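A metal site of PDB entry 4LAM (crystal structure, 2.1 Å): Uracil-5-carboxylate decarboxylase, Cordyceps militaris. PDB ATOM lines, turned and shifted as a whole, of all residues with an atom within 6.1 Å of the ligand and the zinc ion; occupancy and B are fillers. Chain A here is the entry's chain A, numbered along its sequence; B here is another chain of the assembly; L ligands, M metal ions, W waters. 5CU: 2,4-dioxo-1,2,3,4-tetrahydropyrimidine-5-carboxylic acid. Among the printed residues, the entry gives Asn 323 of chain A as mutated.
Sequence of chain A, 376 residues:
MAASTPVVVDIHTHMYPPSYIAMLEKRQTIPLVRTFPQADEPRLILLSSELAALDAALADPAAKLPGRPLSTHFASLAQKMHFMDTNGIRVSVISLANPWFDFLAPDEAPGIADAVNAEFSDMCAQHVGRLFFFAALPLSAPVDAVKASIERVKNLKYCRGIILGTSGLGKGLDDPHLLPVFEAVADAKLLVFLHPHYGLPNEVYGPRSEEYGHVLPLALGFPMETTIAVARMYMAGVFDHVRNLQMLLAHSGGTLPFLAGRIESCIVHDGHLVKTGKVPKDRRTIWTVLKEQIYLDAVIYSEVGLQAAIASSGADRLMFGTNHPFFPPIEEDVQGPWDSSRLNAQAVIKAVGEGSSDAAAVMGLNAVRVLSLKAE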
ATOM      1  N   HIS A  12       0.068 -12.856  10.916  1.00  0.00           N
ATOM      2  CA  HIS A  12       0.394 -13.925   9.985  1.00  0.00           C
ATOM      3  C   HIS A  12      -0.753 -13.997   8.998  1.00  0.00           C
ATOM      4  O   HIS A  12      -1.687 -14.786   9.175  1.00  0.00           O
ATOM      5  CB  HIS A  12       0.583 -15.252  10.727  1.00  0.00           C
ATOM      6  CG  HIS A  12       1.136 -16.352   9.872  1.00  0.00           C
ATOM      7  ND1 HIS A  12       1.947 -17.351  10.393  1.00  0.00           N
ATOM      8  CD2 HIS A  12       1.014 -16.623   8.554  1.00  0.00           C
ATOM      9  CE1 HIS A  12       2.281 -18.190   9.421  1.00  0.00           C
ATOM     10  NE2 HIS A  12       1.733 -17.772   8.295  1.00  0.00           N
ATOM     11  N   HIS A  14      -1.659 -13.228   4.665  1.00  0.00           N
ATOM     12  CA  HIS A  14      -0.944 -13.095   3.407  1.00  0.00           C
ATOM     13  C   HIS A  14      -1.784 -12.535   2.275  1.00  0.00           C
ATOM     14  O   HIS A  14      -3.023 -12.572   2.317  1.00  0.00           O
ATOM     15  CB  HIS A  14      -0.417 -14.462   2.944  1.00  0.00           C
ATOM     16  CG  HIS A  14       0.480 -15.146   3.934  1.00  0.00           C
ATOM     17  ND1 HIS A  14       1.627 -14.558   4.427  1.00  0.00           N
ATOM     18  CD2 HIS A  14       0.407 -16.375   4.493  1.00  0.00           C
ATOM     19  CE1 HIS A  14       2.224 -15.402   5.258  1.00  0.00           C
ATOM     20  NE2 HIS A  14       1.501 -16.507   5.316  1.00  0.00           N
ATOM     21  N   TYR A  16      -1.279 -12.223  -2.337  1.00  0.00           N
ATOM     22  CA  TYR A  16      -0.522 -12.100  -3.574  1.00  0.00           C
ATOM     23  C   TYR A  16      -1.226 -11.006  -4.352  1.00  0.00           C
ATOM     24  O   TYR A  16      -2.352 -11.208  -4.792  1.00  0.00           O
ATOM     25  CB  TYR A  16      -0.571 -13.380  -4.408  1.00  0.00           C
ATOM     26  CG  TYR A  16       0.059 -14.619  -3.801  1.00  0.00           C
ATOM     27  CD1 TYR A  16       1.427 -14.688  -3.581  1.00  0.00           C
ATOM     28  CD2 TYR A  16      -0.709 -15.728  -3.479  1.00  0.00           C
ATOM     29  CE1 TYR A  16       2.008 -15.826  -3.039  1.00  0.00           C
ATOM     30  CE2 TYR A  16      -0.142 -16.866  -2.937  1.00  0.00           C
ATOM     31  CZ  TYR A  16       1.224 -16.907  -2.727  1.00  0.00           C
ATOM     32  OH  TYR A  16       1.797 -18.034  -2.181  1.00  0.00           O
ATOM     33  N   LEU A  46       2.901 -24.032  -5.874  1.00  0.00           N
ATOM     34  CA  LEU A  46       4.019 -23.296  -5.273  1.00  0.00           C
ATOM     35  C   LEU A  46       5.187 -24.165  -4.870  1.00  0.00           C
ATOM     36  O   LEU A  46       6.325 -23.703  -4.807  1.00  0.00           O
ATOM     37  CB  LEU A  46       3.542 -22.559  -4.024  1.00  0.00           C
ATOM     38  CG  LEU A  46       2.388 -21.564  -4.168  1.00  0.00           C
ATOM     39  CD1 LEU A  46       1.947 -21.112  -2.797  1.00  0.00           C
ATOM     40  CD2 LEU A  46       2.805 -20.382  -5.029  1.00  0.00           C
ATOM     41  N   LEU A  47       4.908 -25.434  -4.585  1.00  0.00           N
ATOM     42  CA  LEU A  47       5.819 -26.258  -3.803  1.00  0.00           C
ATOM     43  C   LEU A  47       6.543 -27.325  -4.600  1.00  0.00           C
ATOM     44  O   LEU A  47       6.000 -27.894  -5.554  1.00  0.00           O
ATOM     45  CB  LEU A  47       5.074 -26.933  -2.655  1.00  0.00           C
ATOM     46  CG  LEU A  47       4.174 -26.080  -1.757  1.00  0.00           C
ATOM     47  CD1 LEU A  47       3.596 -26.959  -0.662  1.00  0.00           C
ATOM     48  CD2 LEU A  47       4.926 -24.896  -1.174  1.00  0.00           C
ATOM     49  N   ARG A  68      -3.216 -26.315  -5.107  1.00  0.00           N
ATOM     50  CA  ARG A  68      -4.434 -26.027  -4.346  1.00  0.00           C
ATOM     51  C   ARG A  68      -5.275 -25.010  -5.099  1.00  0.00           C
ATOM     52  O   ARG A  68      -4.749 -24.309  -5.979  1.00  0.00           O
ATOM     53  CB  ARG A  68      -4.058 -25.485  -2.969  1.00  0.00           C
ATOM     54  CG  ARG A  68      -3.445 -26.543  -2.055  1.00  0.00           C
ATOM     55  CD  ARG A  68      -2.745 -25.925  -0.856  1.00  0.00           C
ATOM     56  NE  ARG A  68      -1.510 -25.237  -1.233  1.00  0.00           N
ATOM     57  CZ  ARG A  68      -0.685 -24.652  -0.368  1.00  0.00           C
ATOM     58  NH1 ARG A  68      -0.950 -24.690   0.941  1.00  0.00           N
ATOM     59  NH2 ARG A  68       0.419 -24.043  -0.793  1.00  0.00           N
ATOM     60  N   ALA A  97       3.060 -13.767   0.349  1.00  0.00           N
ATOM     61  CA  ALA A  97       3.215 -15.160   0.729  1.00  0.00           C
ATOM     62  C   ALA A  97       4.384 -15.805  -0.015  1.00  0.00           C
ATOM     63  O   ALA A  97       4.958 -15.214  -0.923  1.00  0.00           O
ATOM     64  CB  ALA A  97       1.930 -15.936   0.475  1.00  0.00           C
ATOM     65  N   ASN A  98       4.726 -17.024   0.396  1.00  0.00           N
ATOM     66  CA  ASN A  98       5.811 -17.772  -0.219  1.00  0.00           C
ATOM     67  C   ASN A  98       5.540 -18.030  -1.689  1.00  0.00           C
ATOM     68  O   ASN A  98       4.393 -18.207  -2.079  1.00  0.00           O
ATOM     69  CB  ASN A  98       6.016 -19.112   0.513  1.00  0.00           C
ATOM     70  CG  ASN A  98       4.718 -19.890   0.689  1.00  0.00           C
ATOM     71  OD1 ASN A  98       3.739 -19.368   1.229  1.00  0.00           O
ATOM     72  ND2 ASN A  98       4.683 -21.128   0.214  1.00  0.00           N
ATOM     73  N   PHE A 193      10.287 -11.527   9.916  1.00  0.00           N
ATOM     74  CA  PHE A 193       9.328 -12.626   9.987  1.00  0.00           C
ATOM     75  C   PHE A 193       9.865 -13.802   9.161  1.00  0.00           C
ATOM     76  O   PHE A 193       9.881 -13.741   7.925  1.00  0.00           O
ATOM     77  CB  PHE A 193       7.979 -12.132   9.444  1.00  0.00           C
ATOM     78  CG  PHE A 193       6.852 -13.141   9.544  1.00  0.00           C
ATOM     79  CD1 PHE A 193       6.910 -14.234  10.394  1.00  0.00           C
ATOM     80  CD2 PHE A 193       5.701 -12.966   8.770  1.00  0.00           C
ATOM     81  CE1 PHE A 193       5.859 -15.139  10.469  1.00  0.00           C
ATOM     82  CE2 PHE A 193       4.649 -13.862   8.842  1.00  0.00           C
ATOM     83  CZ  PHE A 193       4.721 -14.944   9.690  1.00  0.00           C
ATOM     84  N   HIS A 195       9.534 -17.421   7.597  1.00  0.00           N
ATOM     85  CA  HIS A 195       8.391 -18.230   7.173  1.00  0.00           C
ATOM     86  C   HIS A 195       8.865 -19.370   6.278  1.00  0.00           C
ATOM     87  O   HIS A 195       9.768 -19.196   5.464  1.00  0.00           O
ATOM     88  CB  HIS A 195       7.401 -17.339   6.393  1.00  0.00           C
ATOM     89  CG  HIS A 195       6.065 -17.971   6.141  1.00  0.00           C
ATOM     90  ND1 HIS A 195       5.879 -18.989   5.242  1.00  0.00           N
ATOM     91  CD2 HIS A 195       4.836 -17.691   6.650  1.00  0.00           C
ATOM     92  CE1 HIS A 195       4.607 -19.345   5.215  1.00  0.00           C
ATOM     93  NE2 HIS A 195       3.952 -18.561   6.061  1.00  0.00           N
ATOM     94  N   PRO A 196       8.272 -20.559   6.434  1.00  0.00           N
ATOM     95  CA  PRO A 196       8.699 -21.701   5.610  1.00  0.00           C
ATOM     96  C   PRO A 196       8.205 -21.668   4.154  1.00  0.00           C
ATOM     97  O   PRO A 196       7.426 -20.789   3.777  1.00  0.00           O
ATOM     98  CB  PRO A 196       8.099 -22.895   6.346  1.00  0.00           C
ATOM     99  CG  PRO A 196       6.885 -22.340   7.053  1.00  0.00           C
ATOM    100  CD  PRO A 196       7.319 -20.954   7.491  1.00  0.00           C
ATOM    101  N   HIS A 197       8.682 -22.626   3.367  1.00  0.00           N
ATOM    102  CA  HIS A 197       8.283 -22.790   1.960  1.00  0.00           C
ATOM    103  C   HIS A 197       8.961 -23.978   1.293  1.00  0.00           C
ATOM    104  O   HIS A 197       8.309 -24.742   0.582  1.00  0.00           O
ATOM    105  CB  HIS A 197       8.645 -21.565   1.117  1.00  0.00           C
ATOM    106  CG  HIS A 197       8.503 -21.824  -0.356  1.00  0.00           C
ATOM    107  ND1 HIS A 197       7.276 -21.902  -0.977  1.00  0.00           N
ATOM    108  CD2 HIS A 197       9.419 -22.104  -1.311  1.00  0.00           C
ATOM    109  CE1 HIS A 197       7.443 -22.180  -2.258  1.00  0.00           C
ATOM    110  NE2 HIS A 197       8.738 -22.301  -2.482  1.00  0.00           N
ATOM    111  N   LEU A 218       3.018 -29.757   4.528  1.00  0.00           N
ATOM    112  CA  LEU A 218       2.489 -28.586   5.237  1.00  0.00           C
ATOM    113  C   LEU A 218       2.551 -28.752   6.751  1.00  0.00           C
ATOM    114  O   LEU A 218       2.923 -27.830   7.468  1.00  0.00           O
ATOM    115  CB  LEU A 218       1.059 -28.257   4.789  1.00  0.00           C
ATOM    116  CG  LEU A 218       0.900 -27.875   3.318  1.00  0.00           C
ATOM    117  CD1 LEU A 218      -0.541 -27.460   3.013  1.00  0.00           C
ATOM    118  CD2 LEU A 218       1.869 -26.754   2.951  1.00  0.00           C
ATOM    119  N   PHE A 222       7.039 -27.824   6.582  1.00  0.00           N
ATOM    120  CA  PHE A 222       7.120 -26.381   6.894  1.00  0.00           C
ATOM    121  C   PHE A 222       7.711 -26.070   8.281  1.00  0.00           C
ATOM    122  O   PHE A 222       8.717 -25.379   8.372  1.00  0.00           O
ATOM    123  CB  PHE A 222       5.750 -25.704   6.731  1.00  0.00           C
ATOM    124  CG  PHE A 222       5.461 -25.215   5.332  1.00  0.00           C
ATOM    125  CD1 PHE A 222       6.103 -25.776   4.229  1.00  0.00           C
ATOM    126  CD2 PHE A 222       4.551 -24.201   5.116  1.00  0.00           C
ATOM    127  CE1 PHE A 222       5.833 -25.333   2.944  1.00  0.00           C
ATOM    128  CE2 PHE A 222       4.272 -23.738   3.831  1.00  0.00           C
ATOM    129  CZ  PHE A 222       4.913 -24.304   2.745  1.00  0.00           C
ATOM    130  N   ALA A 250       7.354 -18.106  12.269  1.00  0.00           N
ATOM    131  CA  ALA A 250       6.098 -18.701  11.819  1.00  0.00           C
ATOM    132  C   ALA A 250       5.735 -19.960  12.621  1.00  0.00           C
ATOM    133  O   ALA A 250       6.613 -20.725  13.031  1.00  0.00           O
ATOM    134  CB  ALA A 250       6.193 -19.057  10.341  1.00  0.00           C
ATOM    135  N   HIS A 251       4.440 -20.172  12.822  1.00  0.00           N
ATOM    136  CA  HIS A 251       3.927 -21.423  13.391  1.00  0.00           C
ATOM    137  C   HIS A 251       4.542 -21.739  14.752  1.00  0.00           C
ATOM    138  O   HIS A 251       5.006 -22.857  14.987  1.00  0.00           O
ATOM    139  CB  HIS A 251       4.144 -22.570  12.407  1.00  0.00           C
ATOM    140  CG  HIS A 251       3.735 -22.219  11.003  1.00  0.00           C
ATOM    141  ND1 HIS A 251       4.583 -22.313   9.924  1.00  0.00           N
ATOM    142  CD2 HIS A 251       2.568 -21.731  10.524  1.00  0.00           C
ATOM    143  CE1 HIS A 251       3.957 -21.921   8.835  1.00  0.00           C
ATOM    144  NE2 HIS A 251       2.730 -21.558   9.170  1.00  0.00           N
ATOM    145  N   TYR A 301      -2.576 -24.291  16.458  1.00  0.00           N
ATOM    146  CA  TYR A 301      -3.772 -25.137  16.361  1.00  0.00           C
ATOM    147  C   TYR A 301      -4.053 -26.055  17.555  1.00  0.00           C
ATOM    148  O   TYR A 301      -4.792 -27.022  17.419  1.00  0.00           O
ATOM    149  CB  TYR A 301      -3.738 -25.991  15.090  1.00  0.00           C
ATOM    150  CG  TYR A 301      -3.498 -25.185  13.822  1.00  0.00           C
ATOM    151  CD1 TYR A 301      -4.542 -24.537  13.186  1.00  0.00           C
ATOM    152  CD2 TYR A 301      -2.219 -25.084  13.274  1.00  0.00           C
ATOM    153  CE1 TYR A 301      -4.325 -23.791  12.032  1.00  0.00           C
ATOM    154  CE2 TYR A 301      -2.001 -24.348  12.123  1.00  0.00           C
ATOM    155  CZ  TYR A 301      -3.059 -23.716  11.506  1.00  0.00           C
ATOM    156  OH  TYR A 301      -2.834 -22.987  10.365  1.00  0.00           O
ATOM    157  N   ASN A 323      -3.014 -17.046   9.398  1.00  0.00           N
ATOM    158  CA  ASN A 323      -2.570 -17.586   8.114  1.00  0.00           C
ATOM    159  C   ASN A 323      -3.656 -17.496   7.023  1.00  0.00           C
ATOM    160  O   ASN A 323      -3.697 -18.320   6.100  1.00  0.00           O
ATOM    161  CB  ASN A 323      -2.067 -19.019   8.242  1.00  0.00           C
ATOM    162  CG  ASN A 323      -1.320 -19.486   7.009  1.00  0.00           C
ATOM    163  OD1 ASN A 323      -0.527 -18.741   6.431  1.00  0.00           O
ATOM    164  ND2 ASN A 323      -1.579 -20.724   6.595  1.00  0.00           N
ATOM    165  N   PHE A 326      -4.940 -19.104   3.525  1.00  0.00           N
ATOM    166  CA  PHE A 326      -4.674 -20.523   3.329  1.00  0.00           C
ATOM    167  C   PHE A 326      -5.615 -21.343   4.206  1.00  0.00           C
ATOM    168  O   PHE A 326      -6.207 -20.818   5.154  1.00  0.00           O
ATOM    169  CB  PHE A 326      -3.209 -20.839   3.642  1.00  0.00           C
ATOM    170  CG  PHE A 326      -2.244 -20.365   2.599  1.00  0.00           C
ATOM    171  CD1 PHE A 326      -2.007 -21.118   1.457  1.00  0.00           C
ATOM    172  CD2 PHE A 326      -1.580 -19.151   2.732  1.00  0.00           C
ATOM    173  CE1 PHE A 326      -1.114 -20.682   0.479  1.00  0.00           C
ATOM    174  CE2 PHE A 326      -0.680 -18.712   1.761  1.00  0.00           C
ATOM    175  CZ  PHE A 326      -0.458 -19.473   0.635  1.00  0.00           C
ATOM    176  N   PHE A 327      -5.776 -22.611   3.870  1.00  0.00           N
ATOM    177  CA  PHE A 327      -6.650 -23.517   4.625  1.00  0.00           C
ATOM    178  C   PHE A 327      -8.075 -22.992   4.793  1.00  0.00           C
ATOM    179  O   PHE A 327      -8.546 -22.860   5.926  1.00  0.00           O
ATOM    180  CB  PHE A 327      -6.067 -23.809   6.005  1.00  0.00           C
ATOM    181  CG  PHE A 327      -4.674 -24.385   5.983  1.00  0.00           C
ATOM    182  CD1 PHE A 327      -4.462 -25.698   5.570  1.00  0.00           C
ATOM    183  CD2 PHE A 327      -3.588 -23.622   6.378  1.00  0.00           C
ATOM    184  CE1 PHE A 327      -3.187 -26.239   5.555  1.00  0.00           C
ATOM    185  CE2 PHE A 327      -2.300 -24.152   6.361  1.00  0.00           C
ATOM    186  CZ  PHE A 327      -2.096 -25.464   5.955  1.00  0.00           C
ATOM    187  N   ARG B 262      -1.382 -29.124  14.488  1.00  0.00           N
ATOM    188  CA  ARG B 262      -1.148 -28.727  13.094  1.00  0.00           C
ATOM    189  C   ARG B 262      -1.487 -29.881  12.133  1.00  0.00           C
ATOM    190  O   ARG B 262      -2.106 -29.663  11.091  1.00  0.00           O
ATOM    191  CB  ARG B 262       0.307 -28.271  12.891  1.00  0.00           C
ATOM    192  CG  ARG B 262       0.585 -27.749  11.478  1.00  0.00           C
ATOM    193  CD  ARG B 262       2.024 -27.276  11.268  1.00  0.00           C
ATOM    194  NE  ARG B 262       2.177 -26.739   9.905  1.00  0.00           N
ATOM    195  CZ  ARG B 262       1.784 -25.523   9.527  1.00  0.00           C
ATOM    196  NH1 ARG B 262       1.222 -24.693  10.398  1.00  0.00           N
ATOM    197  NH2 ARG B 262       1.940 -25.143   8.265  1.00  0.00           N
HETATM  198  O53 5CU L   1       0.806 -22.762   6.779  1.00  0.00           O
HETATM  199  C51 5CU L   1       1.176 -21.737   6.132  1.00  0.00           C
HETATM  200  O52 5CU L   1       1.567 -20.742   6.776  1.00  0.00           O
HETATM  201  C5  5CU L   1       1.287 -21.803   4.736  1.00  0.00           C
HETATM  202  C4  5CU L   1       1.633 -20.718   3.920  1.00  0.00           C
HETATM  203  O4  5CU L   1       1.801 -19.576   4.356  1.00  0.00           O
HETATM  204  N3  5CU L   1       1.770 -20.915   2.537  1.00  0.00           N
HETATM  205  C2  5CU L   1       1.572 -22.177   1.995  1.00  0.00           C
HETATM  206  O2  5CU L   1       1.691 -22.374   0.782  1.00  0.00           O
HETATM  207  N1  5CU L   1       1.220 -23.231   2.846  1.00  0.00           N
HETATM  208  C6  5CU L   1       1.098 -23.051   4.138  1.00  0.00           C
HETATM  209 ZN    ZN M   1       1.683 -18.620   6.204  1.00  0.00          ZN
HETATM  210  O   HOH W   1      -0.220 -22.483   9.448  1.00  0.00           O
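The guanidinium group (NH2) of Arg 68 lies within hydrogen-bond range of an oxygen (O2) of the ligand.
A ring nitrogen (NE2) of His 251 lies within hydrogen-bond range of an oxygen (O53) of the ligand (3.3 Å).
The guanidinium group of Arg 262 of chain B lies within salt-bridge range of an oxygen (O53) of the ligand (3.0 Å).
The side-chain amide oxygen (OD1) of Asn 98 sits at hydrogen-bond distance from a nitrogen (N3) of the ligand (2.8 Å).
A ring nitrogen (ND1) of His 197 is in hydrogen-bond range of the side-chain amide nitrogen (ND2) of Asn 98 (3.0 Å).
The guanidinium group (NE) of Arg 262 of chain B lies within hydrogen-bond range of the backbone carbonyl oxygen (O) of Leu 218.
OH of Tyr 16 sits at hydrogen-bond distance from O of Asn 98, 2.6 Å away.
Leu 46 touches the ligand.
Leu 218 touches the ligand (CD2 to N1, 3.6 Å).
Phe 222 touches the ligand (CE2 to N1, 3.2 Å).
Phe 326 touches the ligand (CZ to N3, 3.3 Å).
Phe 327 touches the ligand (CE2 to O53, 3.4 Å).
Hydrophobic or aromatic side chains within 4 Å of the ligand: His 12, His 14, Leu 46, His 195, Leu 218, Phe 222, His 251, Phe 326 and Phe 327.
Of the 21 residues printed, 13 come within 4 Å of the ligand.
The nearest printed residue that does not touch the ligand is Leu 47 (4.5 Å).
Four residues have an atom within 4 Å of the zinc ion: His 12, His 14, His 195 and Asn 323.
The nearest printed residue that does not touch the zinc ion is His 251 (4.3 Å).
The zinc ion is bound by O4 of the ligand (2.1 Å), O52 of the ligand (2.2 Å), OD1 of Asn 323 (2.2 Å), NE2 of His 12 (2.3 Å), NE2 of His 195 (2.3 Å) and NE2 of His 14 (2.3 Å).
Water W1 lies within hydrogen-bond range of NH1 of Arg 262 of chain B (2.8 Å), OH of Tyr 301 (2.8 Å), O53 of the ligand (2.9 Å) and NE2 of His 251 (3.1 Å).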
